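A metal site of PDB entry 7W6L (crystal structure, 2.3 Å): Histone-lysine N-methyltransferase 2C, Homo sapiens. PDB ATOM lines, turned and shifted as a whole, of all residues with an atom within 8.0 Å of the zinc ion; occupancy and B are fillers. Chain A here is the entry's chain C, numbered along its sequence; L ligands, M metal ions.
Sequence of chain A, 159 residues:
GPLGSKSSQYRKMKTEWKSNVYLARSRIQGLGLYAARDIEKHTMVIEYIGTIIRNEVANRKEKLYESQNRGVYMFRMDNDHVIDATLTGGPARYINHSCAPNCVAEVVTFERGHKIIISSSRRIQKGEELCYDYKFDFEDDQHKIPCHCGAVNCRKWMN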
ATOM      1  N   ILE A  28      10.299  19.962  -6.075  1.00  0.00           N
ATOM      2  CA  ILE A  28       9.590  18.991  -6.879  1.00  0.00           C
ATOM      3  C   ILE A  28      10.618  18.215  -7.682  1.00  0.00           C
ATOM      4  O   ILE A  28      10.770  17.002  -7.522  1.00  0.00           O
ATOM      5  CB  ILE A  28       8.538  19.681  -7.753  1.00  0.00           C
ATOM      6  CG1 ILE A  28       7.526  20.400  -6.861  1.00  0.00           C
ATOM      7  CG2 ILE A  28       7.873  18.657  -8.634  1.00  0.00           C
ATOM      8  CD1 ILE A  28       6.450  21.131  -7.624  1.00  0.00           C
ATOM      9  N   HIS A  97       5.407  21.303 -12.672  1.00  0.00           N
ATOM     10  CA  HIS A  97       4.031  20.864 -12.656  1.00  0.00           C
ATOM     11  C   HIS A  97       3.616  20.498 -11.235  1.00  0.00           C
ATOM     12  O   HIS A  97       4.429  20.028 -10.438  1.00  0.00           O
ATOM     13  CB  HIS A  97       3.839  19.670 -13.598  1.00  0.00           C
ATOM     14  CG  HIS A  97       2.547  18.944 -13.394  1.00  0.00           C
ATOM     15  ND1 HIS A  97       1.406  19.225 -14.111  1.00  0.00           N
ATOM     16  CD2 HIS A  97       2.219  17.931 -12.555  1.00  0.00           C
ATOM     17  CE1 HIS A  97       0.433  18.424 -13.724  1.00  0.00           C
ATOM     18  NE2 HIS A  97       0.904  17.628 -12.771  1.00  0.00           N
ATOM     19  N   SER A  98       2.336  20.725 -10.926  1.00  0.00           N
ATOM     20  CA  SER A  98       1.807  20.384  -9.612  1.00  0.00           C
ATOM     21  C   SER A  98       0.331  20.020  -9.731  1.00  0.00           C
ATOM     22  O   SER A  98      -0.396  20.563 -10.575  1.00  0.00           O
ATOM     23  CB  SER A  98       1.981  21.531  -8.610  1.00  0.00           C
ATOM     24  OG  SER A  98       1.450  21.203  -7.342  1.00  0.00           O
ATOM     25  N   CYS A  99      -0.086  19.084  -8.873  1.00  0.00           N
ATOM     26  CA  CYS A  99      -1.495  18.735  -8.753  1.00  0.00           C
ATOM     27  C   CYS A  99      -2.284  19.799  -8.000  1.00  0.00           C
ATOM     28  O   CYS A  99      -3.497  19.899  -8.196  1.00  0.00           O
ATOM     29  CB  CYS A  99      -1.638  17.379  -8.067  1.00  0.00           C
ATOM     30  SG  CYS A  99      -0.700  16.023  -8.844  1.00  0.00           S
ATOM     31  N   ALA A 100      -1.605  20.574  -7.150  1.00  0.00           N
ATOM     32  CA  ALA A 100      -2.200  21.702  -6.444  1.00  0.00           C
ATOM     33  C   ALA A 100      -1.589  22.996  -6.993  1.00  0.00           C
ATOM     34  O   ALA A 100      -0.780  23.630  -6.318  1.00  0.00           O
ATOM     35  CB  ALA A 100      -1.973  21.590  -4.938  1.00  0.00           C
ATOM     36  N   PRO A 146       5.935   9.622 -13.567  1.00  0.00           N
ATOM     37  CA  PRO A 146       5.463   9.856 -12.193  1.00  0.00           C
ATOM     38  C   PRO A 146       5.590  11.307 -11.768  1.00  0.00           C
ATOM     39  O   PRO A 146       6.452  12.053 -12.248  1.00  0.00           O
ATOM     40  CB  PRO A 146       6.379   8.960 -11.352  1.00  0.00           C
ATOM     41  CG  PRO A 146       7.157   8.098 -12.342  1.00  0.00           C
ATOM     42  CD  PRO A 146       7.219   8.910 -13.589  1.00  0.00           C
ATOM     43  N   CYS A 147       4.725  11.701 -10.834  1.00  0.00           N
ATOM     44  CA  CYS A 147       4.665  13.055 -10.314  1.00  0.00           C
ATOM     45  C   CYS A 147       5.228  13.112  -8.894  1.00  0.00           C
ATOM     46  O   CYS A 147       4.925  12.246  -8.068  1.00  0.00           O
ATOM     47  CB  CYS A 147       3.216  13.588 -10.307  1.00  0.00           C
ATOM     48  SG  CYS A 147       2.997  15.240  -9.551  1.00  0.00           S
ATOM     49  N   HIS A 148       6.041  14.134  -8.625  1.00  0.00           N
ATOM     50  CA  HIS A 148       6.567  14.399  -7.287  1.00  0.00           C
ATOM     51  C   HIS A 148       6.304  15.840  -6.888  1.00  0.00           C
ATOM     52  O   HIS A 148       7.166  16.513  -6.312  1.00  0.00           O
ATOM     53  CB  HIS A 148       8.058  14.083  -7.198  1.00  0.00           C
ATOM     54  CG  HIS A 148       8.536  13.884  -5.793  1.00  0.00           C
ATOM     55  ND1 HIS A 148       8.772  14.933  -4.926  1.00  0.00           N
ATOM     56  CD2 HIS A 148       8.832  12.750  -5.106  1.00  0.00           C
ATOM     57  CE1 HIS A 148       9.186  14.452  -3.763  1.00  0.00           C
ATOM     58  NE2 HIS A 148       9.230  13.133  -3.850  1.00  0.00           N
ATOM     59  N   CYS A 149       5.108  16.351  -7.199  1.00  0.00           N
ATOM     60  CA  CYS A 149       4.752  17.707  -6.757  1.00  0.00           C
ATOM     61  C   CYS A 149       4.681  17.804  -5.234  1.00  0.00           C
ATOM     62  O   CYS A 149       4.730  18.914  -4.706  1.00  0.00           O
ATOM     63  CB  CYS A 149       3.426  18.136  -7.396  1.00  0.00           C
ATOM     64  SG  CYS A 149       1.921  17.532  -6.583  1.00  0.00           S
ATOM     65  N   GLY A 150       4.550  16.679  -4.536  1.00  0.00           N
ATOM     66  CA  GLY A 150       4.600  16.656  -3.092  1.00  0.00           C
ATOM     67  C   GLY A 150       3.343  17.127  -2.381  1.00  0.00           C
ATOM     68  O   GLY A 150       3.293  17.066  -1.148  1.00  0.00           O
ATOM     69  N   ALA A 151       2.336  17.588  -3.111  1.00  0.00           N
ATOM     70  CA  ALA A 151       1.129  18.110  -2.476  1.00  0.00           C
ATOM     71  C   ALA A 151       0.296  16.983  -1.880  1.00  0.00           C
ATOM     72  O   ALA A 151       0.245  15.864  -2.398  1.00  0.00           O
ATOM     73  CB  ALA A 151       0.286  18.898  -3.468  1.00  0.00           C
ATOM     74  N   VAL A 152      -0.448  17.343  -0.847  1.00  0.00           N
ATOM     75  CA  VAL A 152      -1.451  16.407  -0.268  1.00  0.00           C
ATOM     76  C   VAL A 152      -2.492  16.195  -1.360  1.00  0.00           C
ATOM     77  O   VAL A 152      -2.887  17.184  -1.983  1.00  0.00           O
ATOM     78  CB  VAL A 152      -2.070  17.037   0.984  1.00  0.00           C
ATOM     79  CG1 VAL A 152      -3.379  16.382   1.358  1.00  0.00           C
ATOM     80  CG2 VAL A 152      -1.099  17.006   2.136  1.00  0.00           C
ATOM     81  N   ASN A 153      -2.939  14.961  -1.531  1.00  0.00           N
ATOM     82  CA  ASN A 153      -3.910  14.554  -2.569  1.00  0.00           C
ATOM     83  C   ASN A 153      -3.270  14.639  -3.964  1.00  0.00           C
ATOM     84  O   ASN A 153      -3.959  14.981  -4.908  1.00  0.00           O
ATOM     85  CB  ASN A 153      -5.309  15.146  -2.356  1.00  0.00           C
ATOM     86  CG  ASN A 153      -5.811  15.029  -0.942  1.00  0.00           C
ATOM     87  OD1 ASN A 153      -5.934  13.944  -0.412  1.00  0.00           O
ATOM     88  ND2 ASN A 153      -6.145  16.135  -0.324  1.00  0.00           N
ATOM     89  N   CYS A 154      -1.973  14.344  -4.047  1.00  0.00           N
ATOM     90  CA  CYS A 154      -1.249  14.324  -5.350  1.00  0.00           C
ATOM     91  C   CYS A 154      -1.818  13.164  -6.165  1.00  0.00           C
ATOM     92  O   CYS A 154      -2.114  12.141  -5.604  1.00  0.00           O
ATOM     93  CB  CYS A 154       0.261  14.204  -5.132  1.00  0.00           C
ATOM     94  SG  CYS A 154       1.249  13.767  -6.566  1.00  0.00           S
ATOM     95  N   ARG A 155      -1.929  13.348  -7.465  1.00  0.00           N
ATOM     96  CA  ARG A 155      -2.546  12.359  -8.390  1.00  0.00           C
ATOM     97  C   ARG A 155      -1.589  11.208  -8.665  1.00  0.00           C
ATOM     98  O   ARG A 155      -2.014  10.318  -9.365  1.00  0.00           O
ATOM     99  CB  ARG A 155      -2.955  13.048  -9.692  1.00  0.00           C
ATOM    100  CG  ARG A 155      -4.125  14.017  -9.537  1.00  0.00           C
ATOM    101  CD  ARG A 155      -4.822  14.351 -10.835  1.00  0.00           C
ATOM    102  NE  ARG A 155      -4.034  15.293 -11.586  1.00  0.00           N
ATOM    103  CZ  ARG A 155      -3.988  16.590 -11.347  1.00  0.00           C
ATOM    104  NH1 ARG A 155      -4.729  17.141 -10.420  1.00  0.00           N
ATOM    105  NH2 ARG A 155      -3.204  17.329 -12.072  1.00  0.00           N
ATOM    106  N   LYS A 156      -0.305  11.385  -8.348  1.00  0.00           N
ATOM    107  CA  LYS A 156       0.839  10.444  -8.404  1.00  0.00           C
ATOM    108  C   LYS A 156       1.454  10.360  -9.797  1.00  0.00           C
ATOM    109  O   LYS A 156       2.528   9.862  -9.903  1.00  0.00           O
ATOM    110  CB  LYS A 156       0.531   9.012  -7.962  1.00  0.00           C
ATOM    111  CG  LYS A 156      -0.184   8.830  -6.639  1.00  0.00           C
ATOM    112  CD  LYS A 156      -0.559   7.398  -6.402  1.00  0.00           C
ATOM    113  CE  LYS A 156      -1.204   7.162  -5.051  1.00  0.00           C
ATOM    114  NZ  LYS A 156      -1.045   8.341  -4.171  1.00  0.00           N
ATOM    115  N   TRP A 157       0.766  10.815 -10.822  1.00  0.00           N
ATOM    116  CA  TRP A 157       1.248  10.755 -12.218  1.00  0.00           C
ATOM    117  C   TRP A 157       1.025  12.114 -12.873  1.00  0.00           C
ATOM    118  O   TRP A 157       0.058  12.776 -12.545  1.00  0.00           O
ATOM    119  CB  TRP A 157       0.499   9.667 -12.995  1.00  0.00           C
ATOM    120  CG  TRP A 157       0.483   8.359 -12.288  1.00  0.00           C
ATOM    121  CD1 TRP A 157      -0.457   7.907 -11.416  1.00  0.00           C
ATOM    122  CD2 TRP A 157       1.564   7.432 -12.231  1.00  0.00           C
ATOM    123  NE1 TRP A 157      -0.082   6.705 -10.889  1.00  0.00           N
ATOM    124  CE2 TRP A 157       1.156   6.384 -11.377  1.00  0.00           C
ATOM    125  CE3 TRP A 157       2.807   7.361 -12.859  1.00  0.00           C
ATOM    126  CZ2 TRP A 157       1.960   5.284 -11.123  1.00  0.00           C
ATOM    127  CZ3 TRP A 157       3.592   6.265 -12.615  1.00  0.00           C
ATOM    128  CH2 TRP A 157       3.170   5.244 -11.769  1.00  0.00           C
ATOM    129  N   MET A 158       1.908  12.464 -13.806  1.00  0.00           N
ATOM    130  CA  MET A 158       1.825  13.706 -14.621  1.00  0.00           C
ATOM    131  C   MET A 158       0.956  13.437 -15.859  1.00  0.00           C
ATOM    132  O   MET A 158       0.694  14.364 -16.613  1.00  0.00           O
ATOM    133  CB  MET A 158       3.227  14.169 -15.032  1.00  0.00           C
ATOM    134  CG  MET A 158       4.033  14.753 -13.882  1.00  0.00           C
ATOM    135  SD  MET A 158       5.595  15.471 -14.396  1.00  0.00           S
ATOM    136  CE  MET A 158       5.836  14.603 -15.932  1.00  0.00           C
HETATM  137  N1  LIG L   1      12.356  21.087 -12.875  1.00  0.00           N
HETATM  138  C1  LIG L   1      12.698  21.338 -14.275  1.00  0.00           C
HETATM  139  C2  LIG L   1      11.887  22.511 -14.819  1.00  0.00           C
HETATM  140  C3  LIG L   1      10.536  22.136 -15.437  1.00  0.00           C
HETATM  141  S1  LIG L   1      10.682  21.614 -17.170  1.00  0.00           S
HETATM  142  C4  LIG L   1      14.199  21.597 -14.435  1.00  0.00           C
HETATM  143  O1  LIG L   1      14.694  21.753 -15.547  1.00  0.00           O
HETATM  144  O2  LIG L   1      14.951  21.643 -13.458  1.00  0.00           O
HETATM  145  C5  LIG L   1       9.642  20.153 -16.913  1.00  0.00           C
HETATM  146  C6  LIG L   1      10.429  18.923 -16.449  1.00  0.00           C
HETATM  147  O3  LIG L   1      10.657  18.972 -15.048  1.00  0.00           O
HETATM  148  C7  LIG L   1       9.665  17.640 -16.741  1.00  0.00           C
HETATM  149  O4  LIG L   1      10.105  17.034 -17.930  1.00  0.00           O
HETATM  150  C8  LIG L   1       9.937  16.755 -15.541  1.00  0.00           C
HETATM  151  O5  LIG L   1      11.044  15.917 -15.778  1.00  0.00           O
HETATM  152  C9  LIG L   1      10.311  17.740 -14.439  1.00  0.00           C
HETATM  153  N2  LIG L   1       9.108  17.940 -13.601  1.00  0.00           N
HETATM  154  C10 LIG L   1       8.312  19.057 -13.591  1.00  0.00           C
HETATM  155  N3  LIG L   1       7.311  18.861 -12.713  1.00  0.00           N
HETATM  156  C11 LIG L   1       7.440  17.633 -12.169  1.00  0.00           C
HETATM  157  C12 LIG L   1       6.686  16.938 -11.237  1.00  0.00           C
HETATM  158  N4  LIG L   1       5.608  17.504 -10.693  1.00  0.00           N
HETATM  159  N5  LIG L   1       7.067  15.665 -10.863  1.00  0.00           N
HETATM  160  C13 LIG L   1       8.192  15.095 -11.427  1.00  0.00           C
HETATM  161  N6  LIG L   1       8.938  15.788 -12.363  1.00  0.00           N
HETATM  162  C14 LIG L   1       8.571  17.033 -12.729  1.00  0.00           C
HETATM  163 ZN    ZN M   1       1.404  15.659  -7.884  1.00  0.00          ZN
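A nitrogen (N4) of the ligand sits close to the side-chain sulfur of Cys 147 (3.6 Å).
The backbone NH of His 148 is in hydrogen-bond range of a nitrogen (N5) of the ligand.
A nitrogen (N3) of the ligand sits at hydrogen-bond distance from the backbone NH (N) of His 97, at 3.1 Å.
N4 of the ligand lies within hydrogen-bond range of O of His 97 (2.8 Å).
N of Lys 156 lies close to SG of Cys 154 (3.4 Å).
The side-chain hydroxyl (OG) of Ser 98 sits close to the side-chain sulfur (SG) of Cys 149 (3.8 Å).
N of Ala 151 lies close to SG of Cys 149, 3.5 Å away.
SG of Cys 99 lies close to N of Arg 155 (3.3 Å).
The backbone carbonyl oxygen of Lys 156 lies within hydrogen-bond range of the backbone NH of Cys 147.
Of the 18 residues printed, 4 come within 4 Å of the zinc ion.
The nearest printed residue that does not touch the zinc ion is Arg 155 (4.1 Å).
The zinc ion is bound by the side-chain sulfur of Cys 154, the side-chain sulfur of Cys 149, the side-chain sulfur of Cys 99 and the side-chain sulfur of Cys 147.
The zinc ion has four donor atoms within binding distance.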
